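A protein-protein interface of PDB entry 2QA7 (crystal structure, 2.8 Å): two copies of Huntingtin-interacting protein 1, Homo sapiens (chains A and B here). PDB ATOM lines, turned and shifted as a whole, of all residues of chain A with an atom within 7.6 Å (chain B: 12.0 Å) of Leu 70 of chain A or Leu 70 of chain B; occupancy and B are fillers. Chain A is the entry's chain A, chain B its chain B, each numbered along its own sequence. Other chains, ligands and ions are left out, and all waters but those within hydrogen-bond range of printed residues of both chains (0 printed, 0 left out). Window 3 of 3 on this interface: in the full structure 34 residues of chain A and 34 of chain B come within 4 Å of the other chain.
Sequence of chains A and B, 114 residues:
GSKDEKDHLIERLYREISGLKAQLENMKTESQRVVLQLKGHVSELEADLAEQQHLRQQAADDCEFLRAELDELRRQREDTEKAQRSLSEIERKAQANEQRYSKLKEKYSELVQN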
ATOM      1  N   CYS A  63       9.757  13.695  17.601  1.00  0.00           N
ATOM      2  CA  CYS A  63      10.222  12.543  18.362  1.00  0.00           C
ATOM      3  C   CYS A  63      10.334  11.348  17.442  1.00  0.00           C
ATOM      4  O   CYS A  63      11.208  10.502  17.621  1.00  0.00           O
ATOM      5  CB  CYS A  63       9.271  12.178  19.509  1.00  0.00           C
ATOM      6  SG  CYS A  63       8.531  13.553  20.434  1.00  0.00           S
ATOM      7  N   GLU A  64       9.445  11.272  16.459  1.00  0.00           N
ATOM      8  CA  GLU A  64       9.463  10.164  15.510  1.00  0.00           C
ATOM      9  C   GLU A  64      10.895  10.016  15.022  1.00  0.00           C
ATOM     10  O   GLU A  64      11.481   8.932  15.078  1.00  0.00           O
ATOM     11  CB  GLU A  64       8.532  10.469  14.340  1.00  0.00           C
ATOM     12  CG  GLU A  64       7.815   9.257  13.772  1.00  0.00           C
ATOM     13  CD  GLU A  64       6.731   9.642  12.777  1.00  0.00           C
ATOM     14  OE1 GLU A  64       5.640  10.082  13.209  1.00  0.00           O
ATOM     15  OE2 GLU A  64       6.976   9.516  11.559  1.00  0.00           O
ATOM     16  N   PHE A  65      11.449  11.130  14.563  1.00  0.00           N
ATOM     17  CA  PHE A  65      12.817  11.190  14.081  1.00  0.00           C
ATOM     18  C   PHE A  65      13.780  10.622  15.120  1.00  0.00           C
ATOM     19  O   PHE A  65      14.560   9.727  14.817  1.00  0.00           O
ATOM     20  CB  PHE A  65      13.184  12.636  13.792  1.00  0.00           C
ATOM     21  CG  PHE A  65      14.578  12.817  13.305  1.00  0.00           C
ATOM     22  CD1 PHE A  65      14.886  12.624  11.962  1.00  0.00           C
ATOM     23  CD2 PHE A  65      15.588  13.198  14.188  1.00  0.00           C
ATOM     24  CE1 PHE A  65      16.183  12.813  11.499  1.00  0.00           C
ATOM     25  CE2 PHE A  65      16.893  13.391  13.739  1.00  0.00           C
ATOM     26  CZ  PHE A  65      17.192  13.198  12.389  1.00  0.00           C
ATOM     27  N   LEU A  66      13.740  11.155  16.339  1.00  0.00           N
ATOM     28  CA  LEU A  66      14.606  10.658  17.406  1.00  0.00           C
ATOM     29  C   LEU A  66      14.387   9.161  17.608  1.00  0.00           C
ATOM     30  O   LEU A  66      15.338   8.377  17.709  1.00  0.00           O
ATOM     31  CB  LEU A  66      14.301  11.374  18.715  1.00  0.00           C
ATOM     32  CG  LEU A  66      14.643  12.853  18.767  1.00  0.00           C
ATOM     33  CD1 LEU A  66      14.157  13.410  20.072  1.00  0.00           C
ATOM     34  CD2 LEU A  66      16.135  13.049  18.634  1.00  0.00           C
ATOM     35  N   ARG A  67      13.118   8.779  17.685  1.00  0.00           N
ATOM     36  CA  ARG A  67      12.753   7.392  17.879  1.00  0.00           C
ATOM     37  C   ARG A  67      13.446   6.545  16.823  1.00  0.00           C
ATOM     38  O   ARG A  67      13.862   5.429  17.105  1.00  0.00           O
ATOM     39  CB  ARG A  67      11.229   7.246  17.805  1.00  0.00           C
ATOM     40  CG  ARG A  67      10.690   5.836  18.009  1.00  0.00           C
ATOM     41  CD  ARG A  67      10.584   5.072  16.686  1.00  0.00           C
ATOM     42  NE  ARG A  67       9.735   3.884  16.789  1.00  0.00           N
ATOM     43  CZ  ARG A  67       9.344   3.152  15.748  1.00  0.00           C
ATOM     44  NH1 ARG A  67       9.724   3.480  14.518  1.00  0.00           N
ATOM     45  NH2 ARG A  67       8.566   2.094  15.934  1.00  0.00           N
ATOM     46  N   ALA A  68      13.593   7.078  15.613  1.00  0.00           N
ATOM     47  CA  ALA A  68      14.265   6.335  14.542  1.00  0.00           C
ATOM     48  C   ALA A  68      15.766   6.367  14.774  1.00  0.00           C
ATOM     49  O   ALA A  68      16.457   5.381  14.546  1.00  0.00           O
ATOM     50  CB  ALA A  68      13.942   6.933  13.182  1.00  0.00           C
ATOM     51  N   GLU A  69      16.268   7.509  15.225  1.00  0.00           N
ATOM     52  CA  GLU A  69      17.689   7.639  15.499  1.00  0.00           C
ATOM     53  C   GLU A  69      18.072   6.511  16.445  1.00  0.00           C
ATOM     54  O   GLU A  69      19.096   5.849  16.260  1.00  0.00           O
ATOM     55  CB  GLU A  69      17.980   8.984  16.169  1.00  0.00           C
ATOM     56  CG  GLU A  69      19.211   9.679  15.649  1.00  0.00           C
ATOM     57  CD  GLU A  69      19.120   9.924  14.154  1.00  0.00           C
ATOM     58  OE1 GLU A  69      18.090  10.479  13.715  1.00  0.00           O
ATOM     59  OE2 GLU A  69      20.068   9.564  13.417  1.00  0.00           O
ATOM     60  N   LEU A  70      17.221   6.293  17.447  1.00  0.00           N
ATOM     61  CA  LEU A  70      17.451   5.272  18.454  1.00  0.00           C
ATOM     62  C   LEU A  70      17.361   3.863  17.936  1.00  0.00           C
ATOM     63  O   LEU A  70      18.131   3.003  18.349  1.00  0.00           O
ATOM     64  CB  LEU A  70      16.469   5.424  19.612  1.00  0.00           C
ATOM     65  CG  LEU A  70      16.600   6.672  20.484  1.00  0.00           C
ATOM     66  CD1 LEU A  70      15.787   6.435  21.744  1.00  0.00           C
ATOM     67  CD2 LEU A  70      18.063   6.952  20.840  1.00  0.00           C
ATOM     68  N   ASP A  71      16.410   3.607  17.051  1.00  0.00           N
ATOM     69  CA  ASP A  71      16.276   2.267  16.515  1.00  0.00           C
ATOM     70  C   ASP A  71      17.537   1.899  15.759  1.00  0.00           C
ATOM     71  O   ASP A  71      18.013   0.767  15.847  1.00  0.00           O
ATOM     72  CB  ASP A  71      15.077   2.167  15.580  1.00  0.00           C
ATOM     73  CG  ASP A  71      13.781   2.444  16.280  1.00  0.00           C
ATOM     74  OD1 ASP A  71      13.630   2.002  17.443  1.00  0.00           O
ATOM     75  OD2 ASP A  71      12.913   3.097  15.662  1.00  0.00           O
ATOM     76  N   GLU A  72      18.079   2.867  15.027  1.00  0.00           N
ATOM     77  CA  GLU A  72      19.280   2.638  14.243  1.00  0.00           C
ATOM     78  C   GLU A  72      20.472   2.338  15.137  1.00  0.00           C
ATOM     79  O   GLU A  72      21.204   1.389  14.894  1.00  0.00           O
ATOM     80  CB  GLU A  72      19.574   3.844  13.354  1.00  0.00           C
ATOM     81  CG  GLU A  72      20.537   3.537  12.217  1.00  0.00           C
ATOM     82  CD  GLU A  72      20.149   2.279  11.450  1.00  0.00           C
ATOM     83  OE1 GLU A  72      18.933   2.015  11.309  1.00  0.00           O
ATOM     84  OE2 GLU A  72      21.058   1.562  10.982  1.00  0.00           O
ATOM     85  N   LEU A  73      20.670   3.143  16.171  1.00  0.00           N
ATOM     86  CA  LEU A  73      21.775   2.913  17.092  1.00  0.00           C
ATOM     87  C   LEU A  73      21.630   1.529  17.730  1.00  0.00           C
ATOM     88  O   LEU A  73      22.625   0.840  17.974  1.00  0.00           O
ATOM     89  CB  LEU A  73      21.800   4.001  18.174  1.00  0.00           C
ATOM     90  CG  LEU A  73      22.420   5.362  17.825  1.00  0.00           C
ATOM     91  CD1 LEU A  73      23.927   5.278  17.955  1.00  0.00           C
ATOM     92  CD2 LEU A  73      22.016   5.801  16.415  1.00  0.00           C
ATOM     93  N   ARG A  74      20.392   1.120  17.995  1.00  0.00           N
ATOM     94  CA  ARG A  74      20.149  -0.186  18.587  1.00  0.00           C
ATOM     95  C   ARG A  74      20.465  -1.281  17.565  1.00  0.00           C
ATOM     96  O   ARG A  74      20.971  -2.341  17.916  1.00  0.00           O
ATOM     97  CB  ARG A  74      18.697  -0.300  19.050  1.00  0.00           C
ATOM     98  CG  ARG A  74      18.414  -1.563  19.846  1.00  0.00           C
ATOM     99  CD  ARG A  74      16.961  -1.640  20.283  1.00  0.00           C
ATOM    100  NE  ARG A  74      16.729  -2.791  21.150  1.00  0.00           N
ATOM    101  CZ  ARG A  74      15.553  -3.102  21.686  1.00  0.00           C
ATOM    102  NH1 ARG A  74      14.490  -2.345  21.444  1.00  0.00           N
ATOM    103  NH2 ARG A  74      15.441  -4.169  22.470  1.00  0.00           N
ATOM    104  N   ARG A  75      20.154  -1.011  16.301  1.00  0.00           N
ATOM    105  CA  ARG A  75      20.418  -1.938  15.202  1.00  0.00           C
ATOM    106  C   ARG A  75      21.931  -2.167  15.147  1.00  0.00           C
ATOM    107  O   ARG A  75      22.407  -3.300  15.062  1.00  0.00           O
ATOM    108  CB  ARG A  75      19.940  -1.318  13.887  1.00  0.00           C
ATOM    109  CG  ARG A  75      20.158  -2.172  12.657  1.00  0.00           C
ATOM    110  CD  ARG A  75      19.948  -1.363  11.384  1.00  0.00           C
ATOM    111  NE  ARG A  75      20.472  -2.050  10.206  1.00  0.00           N
ATOM    112  CZ  ARG A  75      20.414  -1.564   8.972  1.00  0.00           C
ATOM    113  NH1 ARG A  75      19.852  -0.383   8.751  1.00  0.00           N
ATOM    114  NH2 ARG A  75      20.917  -2.259   7.960  1.00  0.00           N
ATOM    115  N   GLN A  76      22.675  -1.068  15.198  1.00  0.00           N
ATOM    116  CA  GLN A  76      24.122  -1.109  15.182  1.00  0.00           C
ATOM    117  C   GLN A  76      24.652  -1.970  16.323  1.00  0.00           C
ATOM    118  O   GLN A  76      25.327  -2.961  16.087  1.00  0.00           O
ATOM    119  CB  GLN A  76      24.686   0.303  15.297  1.00  0.00           C
ATOM    120  CG  GLN A  76      25.338   0.820  14.039  1.00  0.00           C
ATOM    121  CD  GLN A  76      24.746   2.134  13.583  1.00  0.00           C
ATOM    122  OE1 GLN A  76      23.589   2.188  13.176  1.00  0.00           O
ATOM    123  NE2 GLN A  76      25.533   3.206  13.658  1.00  0.00           N
ATOM    124  N   ASP B  61       7.399  16.644  26.172  1.00  0.00           N
ATOM    125  CA  ASP B  61       8.106  15.901  27.197  1.00  0.00           C
ATOM    126  C   ASP B  61       8.723  14.671  26.561  1.00  0.00           C
ATOM    127  O   ASP B  61       9.856  14.316  26.860  1.00  0.00           O
ATOM    128  CB  ASP B  61       7.153  15.468  28.321  1.00  0.00           C
ATOM    129  CG  ASP B  61       6.658  16.637  29.155  1.00  0.00           C
ATOM    130  OD1 ASP B  61       7.363  17.671  29.196  1.00  0.00           O
ATOM    131  OD2 ASP B  61       5.579  16.510  29.781  1.00  0.00           O
ATOM    132  N   ASP B  62       7.968  14.015  25.687  1.00  0.00           N
ATOM    133  CA  ASP B  62       8.464  12.824  25.014  1.00  0.00           C
ATOM    134  C   ASP B  62       9.807  13.092  24.355  1.00  0.00           C
ATOM    135  O   ASP B  62      10.823  12.560  24.779  1.00  0.00           O
ATOM    136  CB  ASP B  62       7.474  12.350  23.951  1.00  0.00           C
ATOM    137  CG  ASP B  62       6.423  11.400  24.501  1.00  0.00           C
ATOM    138  OD1 ASP B  62       6.295  11.282  25.739  1.00  0.00           O
ATOM    139  OD2 ASP B  62       5.714  10.773  23.676  1.00  0.00           O
ATOM    140  N   CYS B  63       9.809  13.923  23.320  1.00  0.00           N
ATOM    141  CA  CYS B  63      11.037  14.223  22.607  1.00  0.00           C
ATOM    142  C   CYS B  63      12.157  14.549  23.580  1.00  0.00           C
ATOM    143  O   CYS B  63      13.274  14.060  23.443  1.00  0.00           O
ATOM    144  CB  CYS B  63      10.834  15.391  21.643  1.00  0.00           C
ATOM    145  SG  CYS B  63       9.772  15.158  20.153  1.00  0.00           S
ATOM    146  N   GLU B  64      11.854  15.367  24.576  1.00  0.00           N
ATOM    147  CA  GLU B  64      12.841  15.750  25.575  1.00  0.00           C
ATOM    148  C   GLU B  64      13.473  14.515  26.239  1.00  0.00           C
ATOM    149  O   GLU B  64      14.676  14.486  26.491  1.00  0.00           O
ATOM    150  CB  GLU B  64      12.176  16.652  26.612  1.00  0.00           C
ATOM    151  CG  GLU B  64      13.105  17.344  27.583  1.00  0.00           C
ATOM    152  CD  GLU B  64      12.449  18.566  28.210  1.00  0.00           C
ATOM    153  OE1 GLU B  64      11.270  18.472  28.625  1.00  0.00           O
ATOM    154  OE2 GLU B  64      13.112  19.621  28.288  1.00  0.00           O
ATOM    155  N   PHE B  65      12.674  13.493  26.520  1.00  0.00           N
ATOM    156  CA  PHE B  65      13.221  12.288  27.125  1.00  0.00           C
ATOM    157  C   PHE B  65      13.938  11.457  26.086  1.00  0.00           C
ATOM    158  O   PHE B  65      14.933  10.802  26.384  1.00  0.00           O
ATOM    159  CB  PHE B  65      12.131  11.449  27.769  1.00  0.00           C
ATOM    160  CG  PHE B  65      11.784  11.880  29.154  1.00  0.00           C
ATOM    161  CD1 PHE B  65      10.913  12.937  29.371  1.00  0.00           C
ATOM    162  CD2 PHE B  65      12.331  11.227  30.246  1.00  0.00           C
ATOM    163  CE1 PHE B  65      10.593  13.332  30.665  1.00  0.00           C
ATOM    164  CE2 PHE B  65      12.017  11.614  31.540  1.00  0.00           C
ATOM    165  CZ  PHE B  65      11.148  12.666  31.752  1.00  0.00           C
ATOM    166  N   LEU B  66      13.418  11.466  24.866  1.00  0.00           N
ATOM    167  CA  LEU B  66      14.047  10.722  23.791  1.00  0.00           C
ATOM    168  C   LEU B  66      15.405  11.343  23.538  1.00  0.00           C
ATOM    169  O   LEU B  66      16.405  10.643  23.416  1.00  0.00           O
ATOM    170  CB  LEU B  66      13.201  10.789  22.520  1.00  0.00           C
ATOM    171  CG  LEU B  66      12.047   9.786  22.421  1.00  0.00           C
ATOM    172  CD1 LEU B  66      11.234  10.082  21.198  1.00  0.00           C
ATOM    173  CD2 LEU B  66      12.582   8.375  22.331  1.00  0.00           C
ATOM    174  N   ARG B  67      15.432  12.668  23.477  1.00  0.00           N
ATOM    175  CA  ARG B  67      16.667  13.405  23.233  1.00  0.00           C
ATOM    176  C   ARG B  67      17.700  13.018  24.283  1.00  0.00           C
ATOM    177  O   ARG B  67      18.893  12.930  23.996  1.00  0.00           O
ATOM    178  CB  ARG B  67      16.390  14.904  23.291  1.00  0.00           C
ATOM    179  CG  ARG B  67      17.169  15.729  22.300  1.00  0.00           C
ATOM    180  CD  ARG B  67      16.528  17.097  22.161  1.00  0.00           C
ATOM    181  NE  ARG B  67      15.098  16.983  21.880  1.00  0.00           N
ATOM    182  CZ  ARG B  67      14.139  17.559  22.602  1.00  0.00           C
ATOM    183  NH1 ARG B  67      14.450  18.300  23.660  1.00  0.00           N
ATOM    184  NH2 ARG B  67      12.863  17.383  22.273  1.00  0.00           N
ATOM    185  N   ALA B  68      17.231  12.788  25.503  1.00  0.00           N
ATOM    186  CA  ALA B  68      18.107  12.391  26.595  1.00  0.00           C
ATOM    187  C   ALA B  68      18.609  10.967  26.344  1.00  0.00           C
ATOM    188  O   ALA B  68      19.812  10.737  26.271  1.00  0.00           O
ATOM    189  CB  ALA B  68      17.355  12.467  27.922  1.00  0.00           C
ATOM    190  N   GLU B  69      17.688  10.017  26.198  1.00  0.00           N
ATOM    191  CA  GLU B  69      18.050   8.622  25.946  1.00  0.00           C
ATOM    192  C   GLU B  69      19.091   8.520  24.842  1.00  0.00           C
ATOM    193  O   GLU B  69      19.995   7.690  24.900  1.00  0.00           O
ATOM    194  CB  GLU B  69      16.827   7.812  25.536  1.00  0.00           C
ATOM    195  CG  GLU B  69      17.096   6.335  25.432  1.00  0.00           C
ATOM    196  CD  GLU B  69      15.883   5.578  24.948  1.00  0.00           C
ATOM    197  OE1 GLU B  69      14.756   5.966  25.332  1.00  0.00           O
ATOM    198  OE2 GLU B  69      16.050   4.592  24.193  1.00  0.00           O
ATOM    199  N   LEU B  70      18.948   9.365  23.830  1.00  0.00           N
ATOM    200  CA  LEU B  70      19.884   9.375  22.727  1.00  0.00           C
ATOM    201  C   LEU B  70      21.190   9.966  23.237  1.00  0.00           C
ATOM    202  O   LEU B  70      22.139   9.235  23.514  1.00  0.00           O
ATOM    203  CB  LEU B  70      19.343  10.217  21.570  1.00  0.00           C
ATOM    204  CG  LEU B  70      20.191  10.230  20.297  1.00  0.00           C
ATOM    205  CD1 LEU B  70      20.242   8.829  19.701  1.00  0.00           C
ATOM    206  CD2 LEU B  70      19.595  11.208  19.298  1.00  0.00           C
ATOM    207  N   ASP B  71      21.232  11.288  23.376  1.00  0.00           N
ATOM    208  CA  ASP B  71      22.433  11.965  23.853  1.00  0.00           C
ATOM    209  C   ASP B  71      23.211  11.148  24.884  1.00  0.00           C
ATOM    210  O   ASP B  71      24.426  11.285  24.995  1.00  0.00           O
ATOM    211  CB  ASP B  71      22.072  13.345  24.413  1.00  0.00           C
ATOM    212  CG  ASP B  71      21.787  14.368  23.312  1.00  0.00           C
ATOM    213  OD1 ASP B  71      20.971  14.074  22.411  1.00  0.00           O
ATOM    214  OD2 ASP B  71      22.379  15.467  23.346  1.00  0.00           O
ATOM    215  N   GLU B  72      22.516  10.289  25.629  1.00  0.00           N
ATOM    216  CA  GLU B  72      23.167   9.436  26.622  1.00  0.00           C
ATOM    217  C   GLU B  72      23.998   8.377  25.903  1.00  0.00           C
ATOM    218  O   GLU B  72      25.221   8.492  25.809  1.00  0.00           O
ATOM    219  CB  GLU B  72      22.127   8.743  27.514  1.00  0.00           C
ATOM    220  CG  GLU B  72      22.722   7.805  28.570  1.00  0.00           C
ATOM    221  CD  GLU B  72      23.397   8.543  29.724  1.00  0.00           C
ATOM    222  OE1 GLU B  72      24.125   9.528  29.466  1.00  0.00           O
ATOM    223  OE2 GLU B  72      23.214   8.131  30.891  1.00  0.00           O
ATOM    224  N   LEU B  73      23.328   7.347  25.393  1.00  0.00           N
ATOM    225  CA  LEU B  73      24.010   6.271  24.686  1.00  0.00           C
ATOM    226  C   LEU B  73      25.035   6.793  23.680  1.00  0.00           C
ATOM    227  O   LEU B  73      26.240   6.537  23.899  1.00  0.00           O
ATOM    228  CB  LEU B  73      22.988   5.383  23.976  1.00  0.00           C
ATOM    229  CG  LEU B  73      21.950   4.753  24.904  1.00  0.00           C
ATOM    230  CD1 LEU B  73      21.076   3.782  24.126  1.00  0.00           C
ATOM    231  CD2 LEU B  73      22.657   4.032  26.030  1.00  0.00           C
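SG of Cys 63 of chain A is disulfide-bonded to SG of Cys 63 of chain B, at 2.0 Å.
Among the printed residues, merely in contact across the chains: Cys 63 of chain A with Asp 62 of chain B (3.9 Å), Cys 63 of chain A with Leu 66 of chain B (3.3 Å), Leu 66 of chain A with Cys 63 of chain B (3.5 Å), Leu 66 of chain A with Leu 66 of chain B (3.7 Å), Leu 66 of chain A with Arg 67 of chain B (3.7 Å), Leu 66 of chain A with Leu 70 of chain B (3.98 Å), Glu 69 of chain A with Leu 70 of chain B (3.97 Å), Leu 70 of chain A with Leu 66 of chain B (3.8 Å), Leu 70 of chain A with Glu 69 of chain B (3.1 Å) and Leu 70 of chain A with Leu 70 of chain B (3.1 Å).
Of the printed residues of chain B, Cys 63 of chain A touches Asp 62, Cys 63 and Leu 66.
Leu 66 of chain A touches four residues of chain B.
Ala 68 of chain A touches none of the printed residues of chain B.
Of chain B, only Leu 66 (3.8 Å), Glu 69 (3.1 Å) and Leu 70 (3.1 Å) come within 4 Å of Leu 70 of chain A.
No residue of chain B comes within 4 Å of Asp 71 of chain A.
Leu 73 of chain A touches none of the printed residues of chain B.
Printed residues of chain A within 4 Å of Asp 62 of chain B: Cys 63 (3.9 Å).
Of the printed residues of chain A, Leu 66 of chain B touches Cys 63 (3.3 Å), Leu 66 (3.7 Å) and Leu 70 (3.8 Å).
The nearest residue of chain B that does not touch Leu 70 of chain A is Leu 73 of chain B (5.5 Å).
Hydrophobic or aromatic side chains of chain B within 4 Å of the printed part of chain A: Leu 66 and Leu 70.
Of the 14 printed residues of chain A, 4 touch a printed residue of chain B.
Printed residues of chain A that touch a printed residue of chain B: Cys 63, Leu 66, Glu 69 and Leu 70.
Hydrophobic or aromatic side chains of chain A that line the printed part of chain B: Leu 66 and Leu 70.
Among the printed residues, no Asp or Glu carboxylate lies within 4 Å of a Lys or Arg side-chain nitrogen of the other chain.
Cys 63 of chain A touches its own counterpart, Cys 63 of chain B.
Cys 63 of chain A touches Leu 66 of chain B, and with the chains exchanged Leu 66 of chain A touches Cys 63 of chain B.
Leu 66 of chain A touches Arg 67 of chain B, but with the chains exchanged Arg 67 of chain A does not touch Leu 66 of chain B (4.2 Å).
Glu 69 of chain A touches Leu 70 of chain B, and with the chains exchanged Leu 70 of chain A touches Glu 69 of chain B.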
